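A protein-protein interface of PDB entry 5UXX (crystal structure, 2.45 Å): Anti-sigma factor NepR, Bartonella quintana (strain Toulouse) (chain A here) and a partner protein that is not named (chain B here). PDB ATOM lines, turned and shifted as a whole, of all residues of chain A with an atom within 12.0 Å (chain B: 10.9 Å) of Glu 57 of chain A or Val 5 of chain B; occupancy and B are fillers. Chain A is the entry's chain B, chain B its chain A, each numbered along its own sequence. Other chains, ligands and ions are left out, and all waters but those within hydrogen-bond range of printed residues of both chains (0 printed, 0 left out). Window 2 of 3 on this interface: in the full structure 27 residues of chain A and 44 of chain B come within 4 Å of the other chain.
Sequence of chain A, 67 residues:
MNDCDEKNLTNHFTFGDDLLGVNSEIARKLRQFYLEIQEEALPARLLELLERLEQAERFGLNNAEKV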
ATOM      1  N   GLU A  48      11.998  23.043 -29.154  1.00  0.00           N
ATOM      2  CA  GLU A  48      10.916  22.080 -29.308  1.00  0.00           C
ATOM      3  C   GLU A  48      10.937  21.047 -28.186  1.00  0.00           C
ATOM      4  O   GLU A  48       9.886  20.601 -27.727  1.00  0.00           O
ATOM      5  CB  GLU A  48      11.007  21.382 -30.667  1.00  0.00           C
ATOM      6  N   LEU A  49      12.135  20.678 -27.745  1.00  0.00           N
ATOM      7  CA  LEU A  49      12.289  19.766 -26.617  1.00  0.00           C
ATOM      8  C   LEU A  49      11.696  20.373 -25.353  1.00  0.00           C
ATOM      9  O   LEU A  49      11.021  19.695 -24.578  1.00  0.00           O
ATOM     10  CB  LEU A  49      13.761  19.420 -26.391  1.00  0.00           C
ATOM     11  CG  LEU A  49      14.055  18.641 -25.107  1.00  0.00           C
ATOM     12  CD1 LEU A  49      13.383  17.275 -25.145  1.00  0.00           C
ATOM     13  CD2 LEU A  49      15.551  18.502 -24.881  1.00  0.00           C
ATOM     14  N   LEU A  50      11.954  21.662 -25.158  1.00  0.00           N
ATOM     15  CA  LEU A  50      11.464  22.382 -23.992  1.00  0.00           C
ATOM     16  C   LEU A  50       9.940  22.425 -23.981  1.00  0.00           C
ATOM     17  O   LEU A  50       9.314  22.312 -22.927  1.00  0.00           O
ATOM     18  CB  LEU A  50      12.039  23.800 -23.969  1.00  0.00           C
ATOM     19  CG  LEU A  50      12.047  24.518 -22.622  1.00  0.00           C
ATOM     20  CD1 LEU A  50      12.724  23.652 -21.575  1.00  0.00           C
ATOM     21  CD2 LEU A  50      12.747  25.860 -22.743  1.00  0.00           C
ATOM     22  N   GLU A  51       9.352  22.587 -25.162  1.00  0.00           N
ATOM     23  CA  GLU A  51       7.901  22.600 -25.314  1.00  0.00           C
ATOM     24  C   GLU A  51       7.305  21.241 -24.965  1.00  0.00           C
ATOM     25  O   GLU A  51       6.272  21.152 -24.300  1.00  0.00           O
ATOM     26  CB  GLU A  51       7.507  22.995 -26.738  1.00  0.00           C
ATOM     27  CG  GLU A  51       7.929  24.399 -27.136  1.00  0.00           C
ATOM     28  CD  GLU A  51       7.259  25.467 -26.296  1.00  0.00           C
ATOM     29  OE1 GLU A  51       6.060  25.317 -25.983  1.00  0.00           O
ATOM     30  OE2 GLU A  51       7.933  26.462 -25.953  1.00  0.00           O
ATOM     31  N   ARG A  52       7.966  20.186 -25.429  1.00  0.00           N
ATOM     32  CA  ARG A  52       7.505  18.820 -25.222  1.00  0.00           C
ATOM     33  C   ARG A  52       7.611  18.411 -23.755  1.00  0.00           C
ATOM     34  O   ARG A  52       6.777  17.660 -23.251  1.00  0.00           O
ATOM     35  CB  ARG A  52       8.314  17.865 -26.103  1.00  0.00           C
ATOM     36  CG  ARG A  52       8.044  18.030 -27.592  1.00  0.00           C
ATOM     37  CD  ARG A  52       8.971  17.170 -28.440  1.00  0.00           C
ATOM     38  NE  ARG A  52       8.810  15.740 -28.200  1.00  0.00           N
ATOM     39  CZ  ARG A  52       9.570  14.805 -28.761  1.00  0.00           C
ATOM     40  NH1 ARG A  52      10.545  15.153 -29.590  1.00  0.00           N
ATOM     41  NH2 ARG A  52       9.359  13.524 -28.491  1.00  0.00           N
ATOM     42  N   LEU A  53       8.640  18.909 -23.077  1.00  0.00           N
ATOM     43  CA  LEU A  53       8.796  18.691 -21.642  1.00  0.00           C
ATOM     44  C   LEU A  53       7.667  19.344 -20.852  1.00  0.00           C
ATOM     45  O   LEU A  53       7.153  18.769 -19.892  1.00  0.00           O
ATOM     46  CB  LEU A  53      10.149  19.222 -21.161  1.00  0.00           C
ATOM     47  CG  LEU A  53      11.364  18.358 -21.503  1.00  0.00           C
ATOM     48  CD1 LEU A  53      12.654  19.091 -21.182  1.00  0.00           C
ATOM     49  CD2 LEU A  53      11.295  17.035 -20.757  1.00  0.00           C
ATOM     50  N   GLU A  54       7.287  20.549 -21.265  1.00  0.00           N
ATOM     51  CA  GLU A  54       6.205  21.282 -20.620  1.00  0.00           C
ATOM     52  C   GLU A  54       4.871  20.589 -20.866  1.00  0.00           C
ATOM     53  O   GLU A  54       4.025  20.508 -19.974  1.00  0.00           O
ATOM     54  CB  GLU A  54       6.155  22.724 -21.127  1.00  0.00           C
ATOM     55  CG  GLU A  54       5.073  23.573 -20.485  1.00  0.00           C
ATOM     56  CD  GLU A  54       5.016  24.975 -21.058  1.00  0.00           C
ATOM     57  OE1 GLU A  54       5.313  25.139 -22.260  1.00  0.00           O
ATOM     58  OE2 GLU A  54       4.675  25.914 -20.307  1.00  0.00           O
ATOM     59  N   GLN A  55       4.694  20.094 -22.086  1.00  0.00           N
ATOM     60  CA  GLN A  55       3.477  19.390 -22.474  1.00  0.00           C
ATOM     61  C   GLN A  55       3.285  18.118 -21.653  1.00  0.00           C
ATOM     62  O   GLN A  55       2.163  17.778 -21.276  1.00  0.00           O
ATOM     63  CB  GLN A  55       3.508  19.053 -23.966  1.00  0.00           C
ATOM     64  N   ALA A  56       4.383  17.418 -21.381  1.00  0.00           N
ATOM     65  CA  ALA A  56       4.332  16.187 -20.601  1.00  0.00           C
ATOM     66  C   ALA A  56       3.933  16.467 -19.156  1.00  0.00           C
ATOM     67  O   ALA A  56       3.252  15.660 -18.522  1.00  0.00           O
ATOM     68  CB  ALA A  56       5.675  15.474 -20.651  1.00  0.00           C
ATOM     69  N   GLU A  57       4.367  17.612 -18.639  1.00  0.00           N
ATOM     70  CA  GLU A  57       4.031  18.018 -17.280  1.00  0.00           C
ATOM     71  C   GLU A  57       2.540  18.329 -17.178  1.00  0.00           C
ATOM     72  O   GLU A  57       1.898  18.038 -16.169  1.00  0.00           O
ATOM     73  CB  GLU A  57       4.859  19.233 -16.858  1.00  0.00           C
ATOM     74  CG  GLU A  57       4.735  19.591 -15.385  1.00  0.00           C
ATOM     75  CD  GLU A  57       5.546  20.816 -15.010  1.00  0.00           C
ATOM     76  OE1 GLU A  57       6.122  21.450 -15.919  1.00  0.00           O
ATOM     77  OE2 GLU A  57       5.609  21.144 -13.806  1.00  0.00           O
ATOM     78  N   ARG A  58       2.006  18.923 -18.241  1.00  0.00           N
ATOM     79  CA  ARG A  58       0.602  19.320 -18.313  1.00  0.00           C
ATOM     80  C   ARG A  58      -0.363  18.145 -18.173  1.00  0.00           C
ATOM     81  O   ARG A  58      -1.421  18.274 -17.558  1.00  0.00           O
ATOM     82  CB  ARG A  58       0.331  20.053 -19.629  1.00  0.00           C
ATOM     83  N   PHE A  59       0.003  17.001 -18.743  1.00  0.00           N
ATOM     84  CA  PHE A  59      -0.860  15.825 -18.706  1.00  0.00           C
ATOM     85  C   PHE A  59      -0.743  15.071 -17.385  1.00  0.00           C
ATOM     86  O   PHE A  59      -1.397  14.047 -17.185  1.00  0.00           O
ATOM     87  CB  PHE A  59      -0.531  14.887 -19.871  1.00  0.00           C
ATOM     88  N   GLY A  60       0.090  15.584 -16.485  1.00  0.00           N
ATOM     89  CA  GLY A  60       0.263  14.981 -15.177  1.00  0.00           C
ATOM     90  C   GLY A  60      -0.683  15.569 -14.147  1.00  0.00           C
ATOM     91  O   GLY A  60      -1.578  16.345 -14.483  1.00  0.00           O
ATOM     92  N   VAL B   5       3.961  24.485 -13.724  1.00  0.00           N
ATOM     93  CA  VAL B   5       4.105  25.931 -13.852  1.00  0.00           C
ATOM     94  C   VAL B   5       5.029  26.291 -15.021  1.00  0.00           C
ATOM     95  O   VAL B   5       6.025  25.609 -15.282  1.00  0.00           O
ATOM     96  CB  VAL B   5       4.641  26.569 -12.543  1.00  0.00           C
ATOM     97  CG1 VAL B   5       6.087  26.172 -12.289  1.00  0.00           C
ATOM     98  CG2 VAL B   5       4.486  28.089 -12.578  1.00  0.00           C
ATOM     99  N   LYS B   6       4.669  27.362 -15.723  1.00  0.00           N
ATOM    100  CA  LYS B   6       5.438  27.884 -16.845  1.00  0.00           C
ATOM    101  C   LYS B   6       6.725  28.562 -16.388  1.00  0.00           C
ATOM    102  O   LYS B   6       7.631  28.790 -17.187  1.00  0.00           O
ATOM    103  CB  LYS B   6       4.586  28.867 -17.652  1.00  0.00           C
ATOM    104  N   ASP B   7       6.798  28.866 -15.095  1.00  0.00           N
ATOM    105  CA  ASP B   7       7.910  29.616 -14.514  1.00  0.00           C
ATOM    106  C   ASP B   7       9.290  29.000 -14.722  1.00  0.00           C
ATOM    107  O   ASP B   7      10.218  29.700 -15.127  1.00  0.00           O
ATOM    108  CB  ASP B   7       7.673  29.801 -13.014  1.00  0.00           C
ATOM    109  CG  ASP B   7       6.600  30.831 -12.716  1.00  0.00           C
ATOM    110  OD1 ASP B   7       5.952  31.318 -13.670  1.00  0.00           O
ATOM    111  OD2 ASP B   7       6.398  31.150 -11.527  1.00  0.00           O
ATOM    112  N   PHE B   8       9.436  27.707 -14.448  1.00  0.00           N
ATOM    113  CA  PHE B   8      10.726  27.053 -14.626  1.00  0.00           C
ATOM    114  C   PHE B   8      11.163  27.100 -16.089  1.00  0.00           C
ATOM    115  O   PHE B   8      12.335  27.320 -16.390  1.00  0.00           O
ATOM    116  CB  PHE B   8      10.685  25.607 -14.134  1.00  0.00           C
ATOM    117  CG  PHE B   8      12.006  24.898 -14.241  1.00  0.00           C
ATOM    118  CD1 PHE B   8      13.046  25.217 -13.382  1.00  0.00           C
ATOM    119  CD2 PHE B   8      12.213  23.922 -15.203  1.00  0.00           C
ATOM    120  CE1 PHE B   8      14.266  24.573 -13.477  1.00  0.00           C
ATOM    121  CE2 PHE B   8      13.431  23.274 -15.300  1.00  0.00           C
ATOM    122  CZ  PHE B   8      14.459  23.601 -14.438  1.00  0.00           C
ATOM    123  N   LYS B   9      10.209  26.889 -16.990  1.00  0.00           N
ATOM    124  CA  LYS B   9      10.470  26.951 -18.423  1.00  0.00           C
ATOM    125  C   LYS B   9      10.969  28.326 -18.860  1.00  0.00           C
ATOM    126  O   LYS B   9      11.919  28.436 -19.636  1.00  0.00           O
ATOM    127  CB  LYS B   9       9.206  26.595 -19.206  1.00  0.00           C
ATOM    128  CG  LYS B   9       9.342  26.760 -20.709  1.00  0.00           C
ATOM    129  CD  LYS B   9       7.980  26.850 -21.370  1.00  0.00           C
ATOM    130  CE  LYS B   9       8.103  27.227 -22.836  1.00  0.00           C
ATOM    131  NZ  LYS B   9       6.796  27.125 -23.542  1.00  0.00           N
ATOM    132  N   GLN B  10      10.324  29.372 -18.356  1.00  0.00           N
ATOM    133  CA  GLN B  10      10.677  30.739 -18.717  1.00  0.00           C
ATOM    134  C   GLN B  10      12.045  31.128 -18.165  1.00  0.00           C
ATOM    135  O   GLN B  10      12.774  31.903 -18.784  1.00  0.00           O
ATOM    136  CB  GLN B  10       9.605  31.710 -18.221  1.00  0.00           C
ATOM    137  CG  GLN B  10       8.269  31.553 -18.932  1.00  0.00           C
ATOM    138  CD  GLN B  10       7.252  32.591 -18.509  1.00  0.00           C
ATOM    139  OE1 GLN B  10       6.869  32.662 -17.341  1.00  0.00           O
ATOM    140  NE2 GLN B  10       6.803  33.402 -19.459  1.00  0.00           N
ATOM    141  N   GLU B  11      12.388  30.587 -17.001  1.00  0.00           N
ATOM    142  CA  GLU B  11      13.707  30.803 -16.419  1.00  0.00           C
ATOM    143  C   GLU B  11      14.794  30.146 -17.266  1.00  0.00           C
ATOM    144  O   GLU B  11      15.886  30.694 -17.422  1.00  0.00           O
ATOM    145  CB  GLU B  11      13.761  30.266 -14.985  1.00  0.00           C
ATOM    146  CG  GLU B  11      12.911  31.040 -13.981  1.00  0.00           C
ATOM    147  CD  GLU B  11      13.567  32.326 -13.499  1.00  0.00           C
ATOM    148  OE1 GLU B  11      13.228  32.781 -12.386  1.00  0.00           O
ATOM    149  OE2 GLU B  11      14.411  32.889 -14.228  1.00  0.00           O
ATOM    150  N   LEU B  12      14.487  28.971 -17.808  1.00  0.00           N
ATOM    151  CA  LEU B  12      15.416  28.250 -18.673  1.00  0.00           C
ATOM    152  C   LEU B  12      15.730  29.024 -19.948  1.00  0.00           C
ATOM    153  O   LEU B  12      16.886  29.104 -20.363  1.00  0.00           O
ATOM    154  CB  LEU B  12      14.857  26.874 -19.034  1.00  0.00           C
ATOM    155  CG  LEU B  12      14.974  25.799 -17.954  1.00  0.00           C
ATOM    156  CD1 LEU B  12      14.303  24.519 -18.410  1.00  0.00           C
ATOM    157  CD2 LEU B  12      16.434  25.551 -17.618  1.00  0.00           C
ATOM    158  N   LEU B  13      14.693  29.582 -20.566  1.00  0.00           N
ATOM    159  CA  LEU B  13      14.846  30.346 -21.801  1.00  0.00           C
ATOM    160  C   LEU B  13      15.805  31.522 -21.631  1.00  0.00           C
ATOM    161  O   LEU B  13      16.482  31.920 -22.579  1.00  0.00           O
ATOM    162  CB  LEU B  13      13.483  30.842 -22.287  1.00  0.00           C
ATOM    163  CG  LEU B  13      12.556  29.760 -22.844  1.00  0.00           C
ATOM    164  CD1 LEU B  13      11.137  30.280 -22.990  1.00  0.00           C
ATOM    165  CD2 LEU B  13      13.079  29.250 -24.179  1.00  0.00           C
ATOM    166  N   LEU B  41      19.401  19.955 -20.462  1.00  0.00           N
ATOM    167  CA  LEU B  41      18.015  20.395 -20.362  1.00  0.00           C
ATOM    168  C   LEU B  41      17.110  19.280 -19.845  1.00  0.00           C
ATOM    169  O   LEU B  41      16.227  19.514 -19.020  1.00  0.00           O
ATOM    170  CB  LEU B  41      17.515  20.886 -21.722  1.00  0.00           C
ATOM    171  CG  LEU B  41      16.194  21.655 -21.730  1.00  0.00           C
ATOM    172  CD1 LEU B  41      16.363  23.000 -21.046  1.00  0.00           C
ATOM    173  CD2 LEU B  41      15.683  21.832 -23.151  1.00  0.00           C
ATOM    174  N   ALA B  44      17.995  18.624 -16.116  1.00  0.00           N
ATOM    175  CA  ALA B  44      17.573  19.743 -15.285  1.00  0.00           C
ATOM    176  C   ALA B  44      16.062  19.741 -15.085  1.00  0.00           C
ATOM    177  O   ALA B  44      15.570  20.077 -14.008  1.00  0.00           O
ATOM    178  CB  ALA B  44      18.022  21.058 -15.900  1.00  0.00           C
ATOM    179  N   TRP B  45      15.329  19.363 -16.127  1.00  0.00           N
ATOM    180  CA  TRP B  45      13.876  19.297 -16.043  1.00  0.00           C
ATOM    181  C   TRP B  45      13.435  18.216 -15.062  1.00  0.00           C
ATOM    182  O   TRP B  45      12.463  18.390 -14.329  1.00  0.00           O
ATOM    183  CB  TRP B  45      13.263  19.039 -17.420  1.00  0.00           C
ATOM    184  CG  TRP B  45      11.782  19.258 -17.451  1.00  0.00           C
ATOM    185  CD1 TRP B  45      10.813  18.340 -17.169  1.00  0.00           C
ATOM    186  CD2 TRP B  45      11.101  20.479 -17.763  1.00  0.00           C
ATOM    187  NE1 TRP B  45       9.571  18.911 -17.294  1.00  0.00           N
ATOM    188  CE2 TRP B  45       9.719  20.224 -17.658  1.00  0.00           C
ATOM    189  CE3 TRP B  45      11.525  21.762 -18.125  1.00  0.00           C
ATOM    190  CZ2 TRP B  45       8.758  21.203 -17.901  1.00  0.00           C
ATOM    191  CZ3 TRP B  45      10.568  22.733 -18.367  1.00  0.00           C
ATOM    192  CH2 TRP B  45       9.202  22.447 -18.254  1.00  0.00           C
ATOM    193  N   ALA B  46      14.150  17.097 -15.059  1.00  0.00           N
ATOM    194  CA  ALA B  46      13.831  15.997 -14.160  1.00  0.00           C
ATOM    195  C   ALA B  46      14.198  16.326 -12.714  1.00  0.00           C
ATOM    196  O   ALA B  46      13.498  15.925 -11.784  1.00  0.00           O
ATOM    197  CB  ALA B  46      14.539  14.726 -14.609  1.00  0.00           C
ATOM    198  N   LYS B  47      15.289  17.063 -12.528  1.00  0.00           N
ATOM    199  CA  LYS B  47      15.769  17.392 -11.187  1.00  0.00           C
ATOM    200  C   LYS B  47      15.348  18.784 -10.727  1.00  0.00           C
ATOM    201  O   LYS B  47      15.846  19.282  -9.717  1.00  0.00           O
ATOM    202  CB  LYS B  47      17.295  17.293 -11.136  1.00  0.00           C
ATOM    203  CG  LYS B  47      17.862  15.955 -11.573  1.00  0.00           C
ATOM    204  CD  LYS B  47      19.350  16.072 -11.869  1.00  0.00           C
ATOM    205  CE  LYS B  47      20.170  16.167 -10.593  1.00  0.00           C
ATOM    206  NZ  LYS B  47      21.542  16.691 -10.847  1.00  0.00           N
ATOM    207  N   GLN B  48      14.432  19.406 -11.465  1.00  0.00           N
ATOM    208  CA  GLN B  48      14.031  20.788 -11.204  1.00  0.00           C
ATOM    209  C   GLN B  48      13.508  21.003  -9.784  1.00  0.00           C
ATOM    210  O   GLN B  48      13.639  22.092  -9.228  1.00  0.00           O
ATOM    211  CB  GLN B  48      12.987  21.249 -12.226  1.00  0.00           C
ATOM    212  CG  GLN B  48      11.631  20.581 -12.134  1.00  0.00           C
ATOM    213  CD  GLN B  48      10.660  21.141 -13.154  1.00  0.00           C
ATOM    214  OE1 GLN B  48      10.072  22.204 -12.950  1.00  0.00           O
ATOM    215  NE2 GLN B  48      10.499  20.436 -14.268  1.00  0.00           N
ATOM    216  N   ASP B  49      12.920  19.965  -9.198  1.00  0.00           N
ATOM    217  CA  ASP B  49      12.343  20.075  -7.865  1.00  0.00           C
ATOM    218  C   ASP B  49      13.410  19.990  -6.777  1.00  0.00           C
ATOM    219  O   ASP B  49      13.123  20.210  -5.602  1.00  0.00           O
ATOM    220  CB  ASP B  49      11.292  18.985  -7.645  1.00  0.00           C
ATOM    221  CG  ASP B  49      10.079  19.156  -8.537  1.00  0.00           C
ATOM    222  OD1 ASP B  49       9.336  20.144  -8.358  1.00  0.00           O
ATOM    223  OD2 ASP B  49       9.865  18.294  -9.412  1.00  0.00           O
ATOM    224  N   PHE B  51      16.077  21.872  -7.036  1.00  0.00           N
ATOM    225  CA  PHE B  51      16.706  23.185  -7.077  1.00  0.00           C
ATOM    226  C   PHE B  51      16.378  23.961  -5.809  1.00  0.00           C
ATOM    227  O   PHE B  51      15.212  24.214  -5.506  1.00  0.00           O
ATOM    228  CB  PHE B  51      16.261  23.972  -8.310  1.00  0.00           C
ATOM    229  CG  PHE B  51      16.697  25.409  -8.295  1.00  0.00           C
ATOM    230  CD1 PHE B  51      18.038  25.741  -8.384  1.00  0.00           C
ATOM    231  CD2 PHE B  51      15.765  26.430  -8.191  1.00  0.00           C
ATOM    232  CE1 PHE B  51      18.443  27.062  -8.365  1.00  0.00           C
ATOM    233  CE2 PHE B  51      16.163  27.755  -8.174  1.00  0.00           C
ATOM    234  CZ  PHE B  51      17.504  28.071  -8.262  1.00  0.00           C
ATOM    235  N   MET B  53      15.651  26.805  -3.415  1.00  0.00           N
ATOM    236  CA  MET B  53      15.055  28.127  -3.566  1.00  0.00           C
ATOM    237  C   MET B  53      15.983  29.220  -3.050  1.00  0.00           C
ATOM    238  O   MET B  53      16.555  29.101  -1.967  1.00  0.00           O
ATOM    239  CB  MET B  53      13.712  28.194  -2.833  1.00  0.00           C
ATOM    240  CG  MET B  53      12.633  28.971  -3.570  1.00  0.00           C
ATOM    241  SD  MET B  53      11.893  27.982  -5.079  1.00  0.00           S
ATOM    242  CE  MET B  53      10.701  26.789  -4.097  1.00  0.00           C
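CD2 of Leu 41 of chain B touches CD2 of Leu 49 of chain A, 3.8 Å away. Leu 12 of chain B touches Leu 50 of chain A. Leu 13 of chain B touches Leu 50 of chain A (CD2 to CD2, 3.7 Å). CD1 of Leu 50 of chain A touches CD1 of Leu 41 of chain B, 3.7 Å away. CD1 of Leu 50 of chain A touches CZ3 of Trp 45 of chain B, at 3.97 Å. Leu 53 of chain A touches Trp 45 of chain B. Lys 6 of chain B touches Glu 54 of chain A (CB to OE2, 3.97 Å). CZ2 of Trp 45 of chain B touches N of Glu 54 of chain A (3.7 Å). Glu 57 of chain A touches Val 5 of chain B (OE2 to N, 3.7 Å). Trp 45 of chain B touches Glu 57 of chain A.
Of the 13 printed residues of chain A, 6 touch a printed residue of chain B. Printed residues of chain A that touch a printed residue of chain B: Leu 49, Leu 50, Glu 51, Leu 53, Glu 54 and Glu 57. Hydrophobic or aromatic side chains of chain A within 4 Å of the printed part of chain B: Leu 49, Leu 50 and Leu 53. Along chain A the printed residues that touch a printed residue of chain B span positions 49 to 57. Of the 18 printed residues of chain B, 7 touch a printed residue of chain A. Along chain B the printed residues that touch a printed residue of chain A span positions 5 to 45.
Of the printed residues of chain B, Leu 49 of chain A touches Leu 41 (3.8 Å). Arg 52 of chain A touches none of the printed residues of chain B. No residue of chain B comes within 4 Å of Ala 56 of chain A. Glu 57 of chain A touches just these residues of chain B: Val 5 (3.7 Å) and Trp 45 (3.3 Å). Phe 59 of chain A touches none of the printed residues of chain B. No residue of chain B comes within 4 Å of Gly 60 of chain A. No residue of chain A comes within 4 Å of Asp 7 of chain B. Of the printed residues of chain A, Leu 41 of chain B touches Leu 49 and Leu 50. Of the printed residues of chain A, Trp 45 of chain B touches Leu 50 (3.97 Å), Leu 53 (3.5 Å), Glu 54 (3.7 Å) and Glu 57 (3.3 Å). Phe 51 of chain B touches none of the printed residues of chain A. The nearest residue of chain B that does not touch Glu 57 of chain A is Gln 48 of chain B (4.7 Å).
The side-chain carboxylate of Glu 51 of chain A is in salt-bridge range of the side-chain amino group of Lys 9 of chain B (2.7 Å). NZ of Lys 9 of chain B is in salt-bridge range of OE1 of Glu 54 of chain A, 2.8 Å away.
The backbone carbonyl oxygen (O) of Trp 45 of chain B lies within hydrogen-bond range of the side-chain amide nitrogen (NE2) of Gln 48 of chain B (2.8 Å).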
